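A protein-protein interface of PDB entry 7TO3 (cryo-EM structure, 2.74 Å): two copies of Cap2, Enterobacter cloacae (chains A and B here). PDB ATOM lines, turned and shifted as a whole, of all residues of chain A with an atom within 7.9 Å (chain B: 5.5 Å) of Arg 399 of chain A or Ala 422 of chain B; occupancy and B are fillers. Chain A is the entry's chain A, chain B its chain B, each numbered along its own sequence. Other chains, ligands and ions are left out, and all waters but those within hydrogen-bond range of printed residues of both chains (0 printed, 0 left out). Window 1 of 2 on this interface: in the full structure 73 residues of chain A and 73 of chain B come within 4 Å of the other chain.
NH1 of Arg 399 of chain A lies within hydrogen-bond range of O of Leu 418 of chain B (3.0 Å). NE of Arg 399 of chain A lies close to O of His 421 of chain B (3.3 Å). The guanidinium group (NH2) of Arg 399 of chain A sits at hydrogen-bond distance from the backbone carbonyl oxygen (O) of Leu 423 of chain B, at 3.2 Å.
OE2 of Glu 395 of chain A is in salt-bridge range of NH2 of Arg 399 of chain A. ND1 of His 421 of chain B is in hydrogen-bond range of N of Leu 423 of chain B (2.8 Å).
Among the printed residues, pairs that only touch across the chains: Arg 399 of chain A with Ser 419 of chain B (3.7 Å), Arg 399 of chain A with Ala 422 of chain B (3.96 Å), Arg 442 of chain A with Thr 424 of chain B (3.2 Å) and Ile 443 of chain A with Leu 418 of chain B (3.8 Å).
Of the printed residues of chain B, Arg 399 of chain A touches Leu 418, Ser 419, His 421, Ala 422 and Leu 423. Of the printed residues of chain B, Ile 443 of chain A touches Leu 418. Of the printed residues of chain A, Leu 418 of chain B touches Arg 399 (3.0 Å) and Ile 443 (3.8 Å). Printed residues of chain A within 4 Å of His 421 of chain B: Arg 399. Ala 422 of chain B touches just one residue of chain A: Arg 399 (3.96 Å). Of the printed residues of chain A, Leu 423 of chain B touches Arg 399. Of the printed residues of chain A, Thr 424 of chain B touches Arg 442. The nearest residue of chain B that does not touch Arg 399 of chain A is Ala 557 of chain B (4.2 Å). The nearest printed residue of chain A that does not touch Leu 418 of chain B is Leu 444 of chain A (4.3 Å).
Printed residues of chain B that touch a printed residue of chain A: Leu 418, Ser 419, His 421, Ala 422, Leu 423 and Thr 424. Hydrophobic or aromatic side chains of chain B within 4 Å of the printed part of chain A: Leu 418. Among the printed residues, 7 pairs touch across the chains.
Positions printed for both chains: 392, 395, 422 and 439.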
ATOM      1  N   LEU A 366      14.489 -17.105 -18.651  1.00  0.00           N
ATOM      2  CA  LEU A 366      13.160 -17.667 -18.443  1.00  0.00           C
ATOM      3  C   LEU A 366      12.464 -17.128 -17.202  1.00  0.00           C
ATOM      4  O   LEU A 366      11.239 -16.973 -17.205  1.00  0.00           O
ATOM      5  CB  LEU A 366      13.240 -19.195 -18.349  1.00  0.00           C
ATOM      6  CG  LEU A 366      13.494 -19.956 -19.651  1.00  0.00           C
ATOM      7  CD1 LEU A 366      13.771 -21.424 -19.369  1.00  0.00           C
ATOM      8  CD2 LEU A 366      12.318 -19.802 -20.604  1.00  0.00           C
ATOM      9  N   ARG A 367      13.212 -16.838 -16.139  1.00  0.00           N
ATOM     10  CA  ARG A 367      12.606 -16.410 -14.885  1.00  0.00           C
ATOM     11  C   ARG A 367      13.081 -15.017 -14.494  1.00  0.00           C
ATOM     12  O   ARG A 367      13.422 -14.774 -13.331  1.00  0.00           O
ATOM     13  CB  ARG A 367      12.921 -17.413 -13.773  1.00  0.00           C
ATOM     14  CG  ARG A 367      12.380 -18.811 -14.032  1.00  0.00           C
ATOM     15  CD  ARG A 367      12.861 -19.791 -12.974  1.00  0.00           C
ATOM     16  NE  ARG A 367      12.457 -21.161 -13.271  1.00  0.00           N
ATOM     17  CZ  ARG A 367      13.175 -22.011 -13.993  1.00  0.00           C
ATOM     18  NH1 ARG A 367      14.337 -21.662 -14.520  1.00  0.00           N
ATOM     19  NH2 ARG A 367      12.715 -23.243 -14.189  1.00  0.00           N
ATOM     20  N   GLY A 370      11.334 -13.049 -11.409  1.00  0.00           N
ATOM     21  CA  GLY A 370      11.454 -13.493 -10.034  1.00  0.00           C
ATOM     22  C   GLY A 370      11.904 -14.936  -9.931  1.00  0.00           C
ATOM     23  O   GLY A 370      11.283 -15.830 -10.514  1.00  0.00           O
ATOM     24  N   GLU A 371      12.981 -15.177  -9.187  1.00  0.00           N
ATOM     25  CA  GLU A 371      13.570 -16.503  -9.078  1.00  0.00           C
ATOM     26  C   GLU A 371      14.171 -16.677  -7.691  1.00  0.00           C
ATOM     27  O   GLU A 371      14.385 -15.711  -6.954  1.00  0.00           O
ATOM     28  CB  GLU A 371      14.636 -16.734 -10.157  1.00  0.00           C
ATOM     29  CG  GLU A 371      15.733 -15.681 -10.175  1.00  0.00           C
ATOM     30  CD  GLU A 371      16.579 -15.742 -11.431  1.00  0.00           C
ATOM     31  OE1 GLU A 371      16.261 -16.552 -12.326  1.00  0.00           O
ATOM     32  OE2 GLU A 371      17.564 -14.978 -11.521  1.00  0.00           O
ATOM     33  N   ALA A 372      14.444 -17.930  -7.341  1.00  0.00           N
ATOM     34  CA  ALA A 372      15.032 -18.254  -6.052  1.00  0.00           C
ATOM     35  C   ALA A 372      16.547 -18.054  -6.087  1.00  0.00           C
ATOM     36  O   ALA A 372      17.154 -17.844  -7.141  1.00  0.00           O
ATOM     37  CB  ALA A 372      14.692 -19.689  -5.653  1.00  0.00           C
ATOM     38  N   MET A 392       1.789 -29.898  -4.943  1.00  0.00           N
ATOM     39  CA  MET A 392       1.817 -28.440  -4.988  1.00  0.00           C
ATOM     40  C   MET A 392       3.204 -27.897  -4.669  1.00  0.00           C
ATOM     41  O   MET A 392       3.671 -26.955  -5.324  1.00  0.00           O
ATOM     42  CB  MET A 392       0.779 -27.866  -4.024  1.00  0.00           C
ATOM     43  CG  MET A 392      -0.657 -28.206  -4.392  1.00  0.00           C
ATOM     44  SD  MET A 392      -1.835 -27.773  -3.099  1.00  0.00           S
ATOM     45  CE  MET A 392      -3.362 -28.375  -3.816  1.00  0.00           C
ATOM     46  N   ILE A 393       3.881 -28.480  -3.676  1.00  0.00           N
ATOM     47  CA  ILE A 393       5.230 -28.036  -3.341  1.00  0.00           C
ATOM     48  C   ILE A 393       6.175 -28.273  -4.515  1.00  0.00           C
ATOM     49  O   ILE A 393       7.005 -27.419  -4.847  1.00  0.00           O
ATOM     50  CB  ILE A 393       5.726 -28.733  -2.061  1.00  0.00           C
ATOM     51  CG1 ILE A 393       4.958 -28.214  -0.843  1.00  0.00           C
ATOM     52  CG2 ILE A 393       7.221 -28.522  -1.876  1.00  0.00           C
ATOM     53  CD1 ILE A 393       5.462 -28.755   0.476  1.00  0.00           C
ATOM     54  N   ALA A 394       6.058 -29.436  -5.162  1.00  0.00           N
ATOM     55  CA  ALA A 394       6.904 -29.743  -6.310  1.00  0.00           C
ATOM     56  C   ALA A 394       6.650 -28.774  -7.457  1.00  0.00           C
ATOM     57  O   ALA A 394       7.588 -28.309  -8.115  1.00  0.00           O
ATOM     58  CB  ALA A 394       6.671 -31.186  -6.760  1.00  0.00           C
ATOM     59  N   GLU A 395       5.376 -28.460  -7.716  1.00  0.00           N
ATOM     60  CA  GLU A 395       5.056 -27.514  -8.782  1.00  0.00           C
ATOM     61  C   GLU A 395       5.635 -26.135  -8.489  1.00  0.00           C
ATOM     62  O   GLU A 395       6.221 -25.496  -9.373  1.00  0.00           O
ATOM     63  CB  GLU A 395       3.542 -27.431  -8.977  1.00  0.00           C
ATOM     64  CG  GLU A 395       3.118 -26.587 -10.170  1.00  0.00           C
ATOM     65  CD  GLU A 395       1.631 -26.679 -10.453  1.00  0.00           C
ATOM     66  OE1 GLU A 395       0.934 -27.435  -9.746  1.00  0.00           O
ATOM     67  OE2 GLU A 395       1.159 -25.993 -11.386  1.00  0.00           O
ATOM     68  N   ASN A 396       5.494 -25.664  -7.245  1.00  0.00           N
ATOM     69  CA  ASN A 396       6.049 -24.362  -6.889  1.00  0.00           C
ATOM     70  C   ASN A 396       7.568 -24.352  -7.021  1.00  0.00           C
ATOM     71  O   ASN A 396       8.147 -23.397  -7.554  1.00  0.00           O
ATOM     72  CB  ASN A 396       5.630 -23.982  -5.469  1.00  0.00           C
ATOM     73  CG  ASN A 396       4.135 -23.754  -5.344  1.00  0.00           C
ATOM     74  OD1 ASN A 396       3.408 -23.769  -6.337  1.00  0.00           O
ATOM     75  ND2 ASN A 396       3.669 -23.540  -4.119  1.00  0.00           N
ATOM     76  N   LEU A 397       8.231 -25.413  -6.553  1.00  0.00           N
ATOM     77  CA  LEU A 397       9.686 -25.479  -6.646  1.00  0.00           C
ATOM     78  C   LEU A 397      10.147 -25.500  -8.098  1.00  0.00           C
ATOM     79  O   LEU A 397      11.142 -24.858  -8.450  1.00  0.00           O
ATOM     80  CB  LEU A 397      10.209 -26.705  -5.898  1.00  0.00           C
ATOM     81  CG  LEU A 397      10.137 -26.643  -4.371  1.00  0.00           C
ATOM     82  CD1 LEU A 397      10.581 -27.962  -3.758  1.00  0.00           C
ATOM     83  CD2 LEU A 397      10.977 -25.490  -3.841  1.00  0.00           C
ATOM     84  N   MET A 398       9.438 -26.240  -8.955  1.00  0.00           N
ATOM     85  CA  MET A 398       9.774 -26.245 -10.374  1.00  0.00           C
ATOM     86  C   MET A 398       9.583 -24.864 -10.988  1.00  0.00           C
ATOM     87  O   MET A 398      10.378 -24.437 -11.834  1.00  0.00           O
ATOM     88  CB  MET A 398       8.930 -27.284 -11.112  1.00  0.00           C
ATOM     89  CG  MET A 398       9.306 -27.461 -12.575  1.00  0.00           C
ATOM     90  SD  MET A 398      10.993 -28.058 -12.796  1.00  0.00           S
ATOM     91  CE  MET A 398      10.842 -29.738 -12.194  1.00  0.00           C
ATOM     92  N   ARG A 399       8.535 -24.149 -10.575  1.00  0.00           N
ATOM     93  CA  ARG A 399       8.279 -22.828 -11.133  1.00  0.00           C
ATOM     94  C   ARG A 399       9.228 -21.756 -10.608  1.00  0.00           C
ATOM     95  O   ARG A 399       9.379 -20.717 -11.261  1.00  0.00           O
ATOM     96  CB  ARG A 399       6.832 -22.410 -10.864  1.00  0.00           C
ATOM     97  CG  ARG A 399       5.813 -23.193 -11.672  1.00  0.00           C
ATOM     98  CD  ARG A 399       4.471 -22.483 -11.719  1.00  0.00           C
ATOM     99  NE  ARG A 399       3.405 -23.375 -12.159  1.00  0.00           N
ATOM    100  CZ  ARG A 399       3.008 -23.501 -13.418  1.00  0.00           C
ATOM    101  NH1 ARG A 399       3.570 -22.804 -14.392  1.00  0.00           N
ATOM    102  NH2 ARG A 399       2.023 -24.346 -13.706  1.00  0.00           N
ATOM    103  N   ILE A 400       9.872 -21.970  -9.456  1.00  0.00           N
ATOM    104  CA  ILE A 400      10.770 -20.954  -8.907  1.00  0.00           C
ATOM    105  C   ILE A 400      12.241 -21.200  -9.227  1.00  0.00           C
ATOM    106  O   ILE A 400      13.080 -20.351  -8.889  1.00  0.00           O
ATOM    107  CB  ILE A 400      10.598 -20.802  -7.379  1.00  0.00           C
ATOM    108  CG1 ILE A 400      11.075 -22.061  -6.651  1.00  0.00           C
ATOM    109  CG2 ILE A 400       9.156 -20.454  -7.031  1.00  0.00           C
ATOM    110  CD1 ILE A 400      11.027 -21.943  -5.144  1.00  0.00           C
ATOM    111  N   GLY A 401      12.584 -22.319  -9.861  1.00  0.00           N
ATOM    112  CA  GLY A 401      13.957 -22.510 -10.289  1.00  0.00           C
ATOM    113  C   GLY A 401      14.560 -23.880 -10.050  1.00  0.00           C
ATOM    114  O   GLY A 401      15.430 -24.312 -10.812  1.00  0.00           O
ATOM    115  N   VAL A 402      14.123 -24.574  -8.999  1.00  0.00           N
ATOM    116  CA  VAL A 402      14.656 -25.897  -8.691  1.00  0.00           C
ATOM    117  C   VAL A 402      14.192 -26.875  -9.762  1.00  0.00           C
ATOM    118  O   VAL A 402      12.992 -27.138  -9.900  1.00  0.00           O
ATOM    119  CB  VAL A 402      14.229 -26.363  -7.288  1.00  0.00           C
ATOM    120  CG1 VAL A 402      14.730 -27.774  -7.023  1.00  0.00           C
ATOM    121  CG2 VAL A 402      14.747 -25.400  -6.230  1.00  0.00           C
ATOM    122  N   VAL A 403      15.137 -27.422 -10.523  1.00  0.00           N
ATOM    123  CA  VAL A 403      14.808 -28.253 -11.672  1.00  0.00           C
ATOM    124  C   VAL A 403      15.159 -29.723 -11.476  1.00  0.00           C
ATOM    125  O   VAL A 403      14.565 -30.574 -12.155  1.00  0.00           O
ATOM    126  CB  VAL A 403      15.476 -27.716 -12.956  1.00  0.00           C
ATOM    127  CG1 VAL A 403      14.934 -26.338 -13.301  1.00  0.00           C
ATOM    128  CG2 VAL A 403      16.988 -27.675 -12.792  1.00  0.00           C
ATOM    129  N   GLN A 405      14.631 -32.715  -9.537  1.00  0.00           N
ATOM    130  CA  GLN A 405      13.710 -33.240  -8.541  1.00  0.00           C
ATOM    131  C   GLN A 405      13.414 -34.709  -8.804  1.00  0.00           C
ATOM    132  O   GLN A 405      13.368 -35.161  -9.952  1.00  0.00           O
ATOM    133  CB  GLN A 405      12.393 -32.452  -8.524  1.00  0.00           C
ATOM    134  CG  GLN A 405      12.546 -30.984  -8.169  1.00  0.00           C
ATOM    135  CD  GLN A 405      11.241 -30.223  -8.279  1.00  0.00           C
ATOM    136  OE1 GLN A 405      10.167 -30.818  -8.365  1.00  0.00           O
ATOM    137  NE2 GLN A 405      11.327 -28.897  -8.282  1.00  0.00           N
ATOM    138  N   ALA A 422      -3.031 -31.194  -7.623  1.00  0.00           N
ATOM    139  CA  ALA A 422      -2.471 -30.350  -8.667  1.00  0.00           C
ATOM    140  C   ALA A 422      -2.649 -30.904 -10.080  1.00  0.00           C
ATOM    141  O   ALA A 422      -2.240 -30.236 -11.038  1.00  0.00           O
ATOM    142  CB  ALA A 422      -0.979 -30.106  -8.394  1.00  0.00           C
ATOM    143  N   HIS A 439       3.843 -33.819 -15.540  1.00  0.00           N
ATOM    144  CA  HIS A 439       3.325 -32.461 -15.405  1.00  0.00           C
ATOM    145  C   HIS A 439       4.445 -31.472 -15.102  1.00  0.00           C
ATOM    146  O   HIS A 439       4.462 -30.359 -15.642  1.00  0.00           O
ATOM    147  CB  HIS A 439       2.256 -32.413 -14.315  1.00  0.00           C
ATOM    148  CG  HIS A 439       1.951 -31.031 -13.827  1.00  0.00           C
ATOM    149  ND1 HIS A 439       1.063 -30.196 -14.468  1.00  0.00           N
ATOM    150  CD2 HIS A 439       2.415 -30.339 -12.760  1.00  0.00           C
ATOM    151  CE1 HIS A 439       0.993 -29.047 -13.818  1.00  0.00           C
ATOM    152  NE2 HIS A 439       1.804 -29.109 -12.777  1.00  0.00           N
ATOM    153  N   LEU A 440       5.387 -31.858 -14.238  1.00  0.00           N
ATOM    154  CA  LEU A 440       6.528 -30.999 -13.945  1.00  0.00           C
ATOM    155  C   LEU A 440       7.404 -30.789 -15.173  1.00  0.00           C
ATOM    156  O   LEU A 440       7.880 -29.673 -15.409  1.00  0.00           O
ATOM    157  CB  LEU A 440       7.353 -31.589 -12.802  1.00  0.00           C
ATOM    158  CG  LEU A 440       6.701 -31.580 -11.418  1.00  0.00           C
ATOM    159  CD1 LEU A 440       7.604 -32.244 -10.390  1.00  0.00           C
ATOM    160  CD2 LEU A 440       6.356 -30.161 -10.999  1.00  0.00           C
ATOM    161  N   ARG A 442       6.432 -30.685 -18.152  1.00  0.00           N
ATOM    162  CA  ARG A 442       5.729 -29.845 -19.115  1.00  0.00           C
ATOM    163  C   ARG A 442       5.611 -28.386 -18.679  1.00  0.00           C
ATOM    164  O   ARG A 442       4.760 -27.666 -19.209  1.00  0.00           O
ATOM    165  CB  ARG A 442       4.334 -30.406 -19.394  1.00  0.00           C
ATOM    166  CG  ARG A 442       4.326 -31.750 -20.091  1.00  0.00           C
ATOM    167  CD  ARG A 442       2.904 -32.192 -20.377  1.00  0.00           C
ATOM    168  NE  ARG A 442       2.831 -33.596 -20.762  1.00  0.00           N
ATOM    169  CZ  ARG A 442       1.711 -34.221 -21.095  1.00  0.00           C
ATOM    170  NH1 ARG A 442       0.546 -33.594 -21.104  1.00  0.00           N
ATOM    171  NH2 ARG A 442       1.761 -35.507 -21.431  1.00  0.00           N
ATOM    172  N   ILE A 443       6.442 -27.925 -17.745  1.00  0.00           N
ATOM    173  CA  ILE A 443       6.287 -26.572 -17.214  1.00  0.00           C
ATOM    174  C   ILE A 443       7.190 -25.585 -17.945  1.00  0.00           C
ATOM    175  O   ILE A 443       6.705 -24.639 -18.577  1.00  0.00           O
ATOM    176  CB  ILE A 443       6.558 -26.536 -15.698  1.00  0.00           C
ATOM    177  CG1 ILE A 443       5.445 -27.265 -14.944  1.00  0.00           C
ATOM    178  CG2 ILE A 443       6.670 -25.098 -15.211  1.00  0.00           C
ATOM    179  CD1 ILE A 443       5.536 -27.136 -13.440  1.00  0.00           C
ATOM    180  N   LEU A 444       8.498 -25.786 -17.863  1.00  0.00           N
ATOM    181  CA  LEU A 444       9.480 -24.875 -18.428  1.00  0.00           C
ATOM    182  C   LEU A 444      10.528 -25.662 -19.198  1.00  0.00           C
ATOM    183  O   LEU A 444      10.756 -26.844 -18.921  1.00  0.00           O
ATOM    184  CB  LEU A 444      10.144 -24.032 -17.327  1.00  0.00           C
ATOM    185  CG  LEU A 444       9.333 -22.814 -16.873  1.00  0.00           C
ATOM    186  CD1 LEU A 444       9.958 -22.157 -15.653  1.00  0.00           C
ATOM    187  CD2 LEU A 444       9.183 -21.808 -18.007  1.00  0.00           C
ATOM    188  N   SER B 391      -6.161 -16.764 -12.771  1.00  0.00           N
ATOM    189  CA  SER B 391      -6.164 -18.187 -13.096  1.00  0.00           C
ATOM    190  C   SER B 391      -6.140 -19.050 -11.841  1.00  0.00           C
ATOM    191  O   SER B 391      -6.892 -20.029 -11.745  1.00  0.00           O
ATOM    192  CB  SER B 391      -4.975 -18.522 -13.995  1.00  0.00           C
ATOM    193  OG  SER B 391      -3.748 -18.214 -13.357  1.00  0.00           O
ATOM    194  N   MET B 392      -5.292 -18.704 -10.870  1.00  0.00           N
ATOM    195  CA  MET B 392      -5.231 -19.464  -9.626  1.00  0.00           C
ATOM    196  C   MET B 392      -6.536 -19.361  -8.844  1.00  0.00           C
ATOM    197  O   MET B 392      -7.012 -20.364  -8.293  1.00  0.00           O
ATOM    198  CB  MET B 392      -4.056 -18.982  -8.775  1.00  0.00           C
ATOM    199  CG  MET B 392      -2.697 -19.231  -9.410  1.00  0.00           C
ATOM    200  SD  MET B 392      -1.352 -18.404  -8.538  1.00  0.00           S
ATOM    201  CE  MET B 392       0.041 -18.831  -9.579  1.00  0.00           C
ATOM    202  N   GLU B 395      -9.072 -21.575 -10.571  1.00  0.00           N
ATOM    203  CA  GLU B 395      -8.816 -22.988 -10.306  1.00  0.00           C
ATOM    204  C   GLU B 395      -9.269 -23.377  -8.903  1.00  0.00           C
ATOM    205  O   GLU B 395      -9.910 -24.420  -8.714  1.00  0.00           O
ATOM    206  CB  GLU B 395      -7.332 -23.300 -10.498  1.00  0.00           C
ATOM    207  CG  GLU B 395      -6.994 -24.780 -10.395  1.00  0.00           C
ATOM    208  CD  GLU B 395      -5.558 -25.082 -10.779  1.00  0.00           C
ATOM    209  OE1 GLU B 395      -4.834 -24.142 -11.167  1.00  0.00           O
ATOM    210  OE2 GLU B 395      -5.153 -26.260 -10.690  1.00  0.00           O
ATOM    211  N   LEU B 418       4.618 -18.256 -17.681  1.00  0.00           N
ATOM    212  CA  LEU B 418       4.582 -19.536 -16.984  1.00  0.00           C
ATOM    213  C   LEU B 418       5.457 -19.560 -15.738  1.00  0.00           C
ATOM    214  O   LEU B 418       5.368 -20.523 -14.968  1.00  0.00           O
ATOM    215  CB  LEU B 418       5.003 -20.657 -17.937  1.00  0.00           C
ATOM    216  CG  LEU B 418       4.194 -20.753 -19.232  1.00  0.00           C
ATOM    217  CD1 LEU B 418       4.769 -21.818 -20.152  1.00  0.00           C
ATOM    218  CD2 LEU B 418       2.729 -21.028 -18.934  1.00  0.00           C
ATOM    219  N   SER B 419       6.296 -18.542 -15.521  1.00  0.00           N
ATOM    220  CA  SER B 419       7.016 -18.448 -14.255  1.00  0.00           C
ATOM    221  C   SER B 419       6.055 -18.273 -13.086  1.00  0.00           C
ATOM    222  O   SER B 419       6.288 -18.827 -12.006  1.00  0.00           O
ATOM    223  CB  SER B 419       8.021 -17.297 -14.299  1.00  0.00           C
ATOM    224  OG  SER B 419       7.364 -16.046 -14.390  1.00  0.00           O
ATOM    225  N   ARG B 420       4.971 -17.510 -13.278  1.00  0.00           N
ATOM    226  CA  ARG B 420       3.912 -17.379 -12.283  1.00  0.00           C
ATOM    227  C   ARG B 420       2.559 -17.543 -12.990  1.00  0.00           C
ATOM    228  O   ARG B 420       1.919 -16.595 -13.443  1.00  0.00           O
ATOM    229  CB  ARG B 420       4.013 -16.052 -11.517  1.00  0.00           C
ATOM    230  CG  ARG B 420       3.826 -14.795 -12.361  1.00  0.00           C
ATOM    231  CD  ARG B 420       3.999 -13.513 -11.582  1.00  0.00           C
ATOM    232  NE  ARG B 420       3.708 -12.377 -12.446  1.00  0.00           N
ATOM    233  CZ  ARG B 420       4.613 -11.793 -13.218  1.00  0.00           C
ATOM    234  NH1 ARG B 420       5.880 -12.159 -13.190  1.00  0.00           N
ATOM    235  NH2 ARG B 420       4.236 -10.820 -14.040  1.00  0.00           N
ATOM    236  N   HIS B 421       2.090 -18.787 -13.109  1.00  0.00           N
ATOM    237  CA  HIS B 421       0.805 -18.994 -13.761  1.00  0.00           C
ATOM    238  C   HIS B 421       0.331 -20.407 -13.435  1.00  0.00           C
ATOM    239  O   HIS B 421       1.046 -21.198 -12.811  1.00  0.00           O
ATOM    240  CB  HIS B 421       0.925 -18.723 -15.276  1.00  0.00           C
ATOM    241  CG  HIS B 421      -0.380 -18.720 -16.009  1.00  0.00           C
ATOM    242  ND1 HIS B 421      -0.974 -19.852 -16.530  1.00  0.00           N
ATOM    243  CD2 HIS B 421      -1.208 -17.689 -16.309  1.00  0.00           C
ATOM    244  CE1 HIS B 421      -2.113 -19.521 -17.115  1.00  0.00           C
ATOM    245  NE2 HIS B 421      -2.280 -18.215 -16.990  1.00  0.00           N
ATOM    246  N   ALA B 422      -0.902 -20.710 -13.835  1.00  0.00           N
ATOM    247  CA  ALA B 422      -1.523 -21.995 -13.550  1.00  0.00           C
ATOM    248  C   ALA B 422      -1.543 -22.957 -14.737  1.00  0.00           C
ATOM    249  O   ALA B 422      -2.015 -24.090 -14.578  1.00  0.00           O
ATOM    250  CB  ALA B 422      -2.955 -21.778 -13.039  1.00  0.00           C
ATOM    251  N   LEU B 423      -1.055 -22.547 -15.910  1.00  0.00           N
ATOM    252  CA  LEU B 423      -1.021 -23.399 -17.090  1.00  0.00           C
ATOM    253  C   LEU B 423       0.421 -23.787 -17.417  1.00  0.00           C
ATOM    254  O   LEU B 423       1.353 -23.489 -16.663  1.00  0.00           O
ATOM    255  CB  LEU B 423      -1.697 -22.710 -18.281  1.00  0.00           C
ATOM    256  CG  LEU B 423      -3.192 -22.406 -18.259  1.00  0.00           C
ATOM    257  CD1 LEU B 423      -3.553 -21.581 -19.477  1.00  0.00           C
ATOM    258  CD2 LEU B 423      -4.024 -23.682 -18.215  1.00  0.00           C
ATOM    259  N   THR B 424       0.600 -24.445 -18.559  1.00  0.00           N
ATOM    260  CA  THR B 424       1.883 -25.031 -18.931  1.00  0.00           C
ATOM    261  C   THR B 424       2.242 -24.601 -20.353  1.00  0.00           C
ATOM    262  O   THR B 424       1.611 -23.721 -20.953  1.00  0.00           O
ATOM    263  CB  THR B 424       1.823 -26.557 -18.778  1.00  0.00           C
ATOM    264  OG1 THR B 424       0.714 -27.073 -19.528  1.00  0.00           O
ATOM    265  CG2 THR B 424       1.657 -26.944 -17.317  1.00  0.00           C
ATOM    266  N   LEU B 436      -7.588 -21.237 -20.150  1.00  0.00           N
ATOM    267  CA  LEU B 436      -8.005 -21.370 -18.760  1.00  0.00           C
ATOM    268  C   LEU B 436      -9.345 -22.088 -18.653  1.00  0.00           C
ATOM    269  O   LEU B 436      -9.548 -22.904 -17.747  1.00  0.00           O
ATOM    270  CB  LEU B 436      -8.076 -19.996 -18.093  1.00  0.00           C
ATOM    271  CG  LEU B 436      -8.351 -20.019 -16.588  1.00  0.00           C
ATOM    272  CD1 LEU B 436      -7.247 -20.767 -15.856  1.00  0.00           C
ATOM    273  CD2 LEU B 436      -8.499 -18.607 -16.042  1.00  0.00           C
ATOM    274  N   HIS B 439      -8.788 -25.802 -19.193  1.00  0.00           N
ATOM    275  CA  HIS B 439      -8.173 -26.393 -18.008  1.00  0.00           C
ATOM    276  C   HIS B 439      -9.186 -26.545 -16.878  1.00  0.00           C
ATOM    277  O   HIS B 439      -9.194 -27.561 -16.174  1.00  0.00           O
ATOM    278  CB  HIS B 439      -6.986 -25.546 -17.556  1.00  0.00           C
ATOM    279  CG  HIS B 439      -6.539 -25.828 -16.155  1.00  0.00           C
ATOM    280  ND1 HIS B 439      -5.678 -26.857 -15.842  1.00  0.00           N
ATOM    281  CD2 HIS B 439      -6.833 -25.214 -14.984  1.00  0.00           C
ATOM    282  CE1 HIS B 439      -5.461 -26.867 -14.539  1.00  0.00           C
ATOM    283  NE2 HIS B 439      -6.150 -25.880 -13.996  1.00  0.00           N
ATOM    284  N   ALA B 557       6.240 -17.299  -7.570  1.00  0.00           N
ATOM    285  CA  ALA B 557       5.021 -18.100  -7.657  1.00  0.00           C
ATOM    286  C   ALA B 557       4.371 -18.295  -6.292  1.00  0.00           C
ATOM    287  O   ALA B 557       3.140 -18.248  -6.170  1.00  0.00           O
ATOM    288  CB  ALA B 557       5.330 -19.452  -8.300  1.00  0.00           C
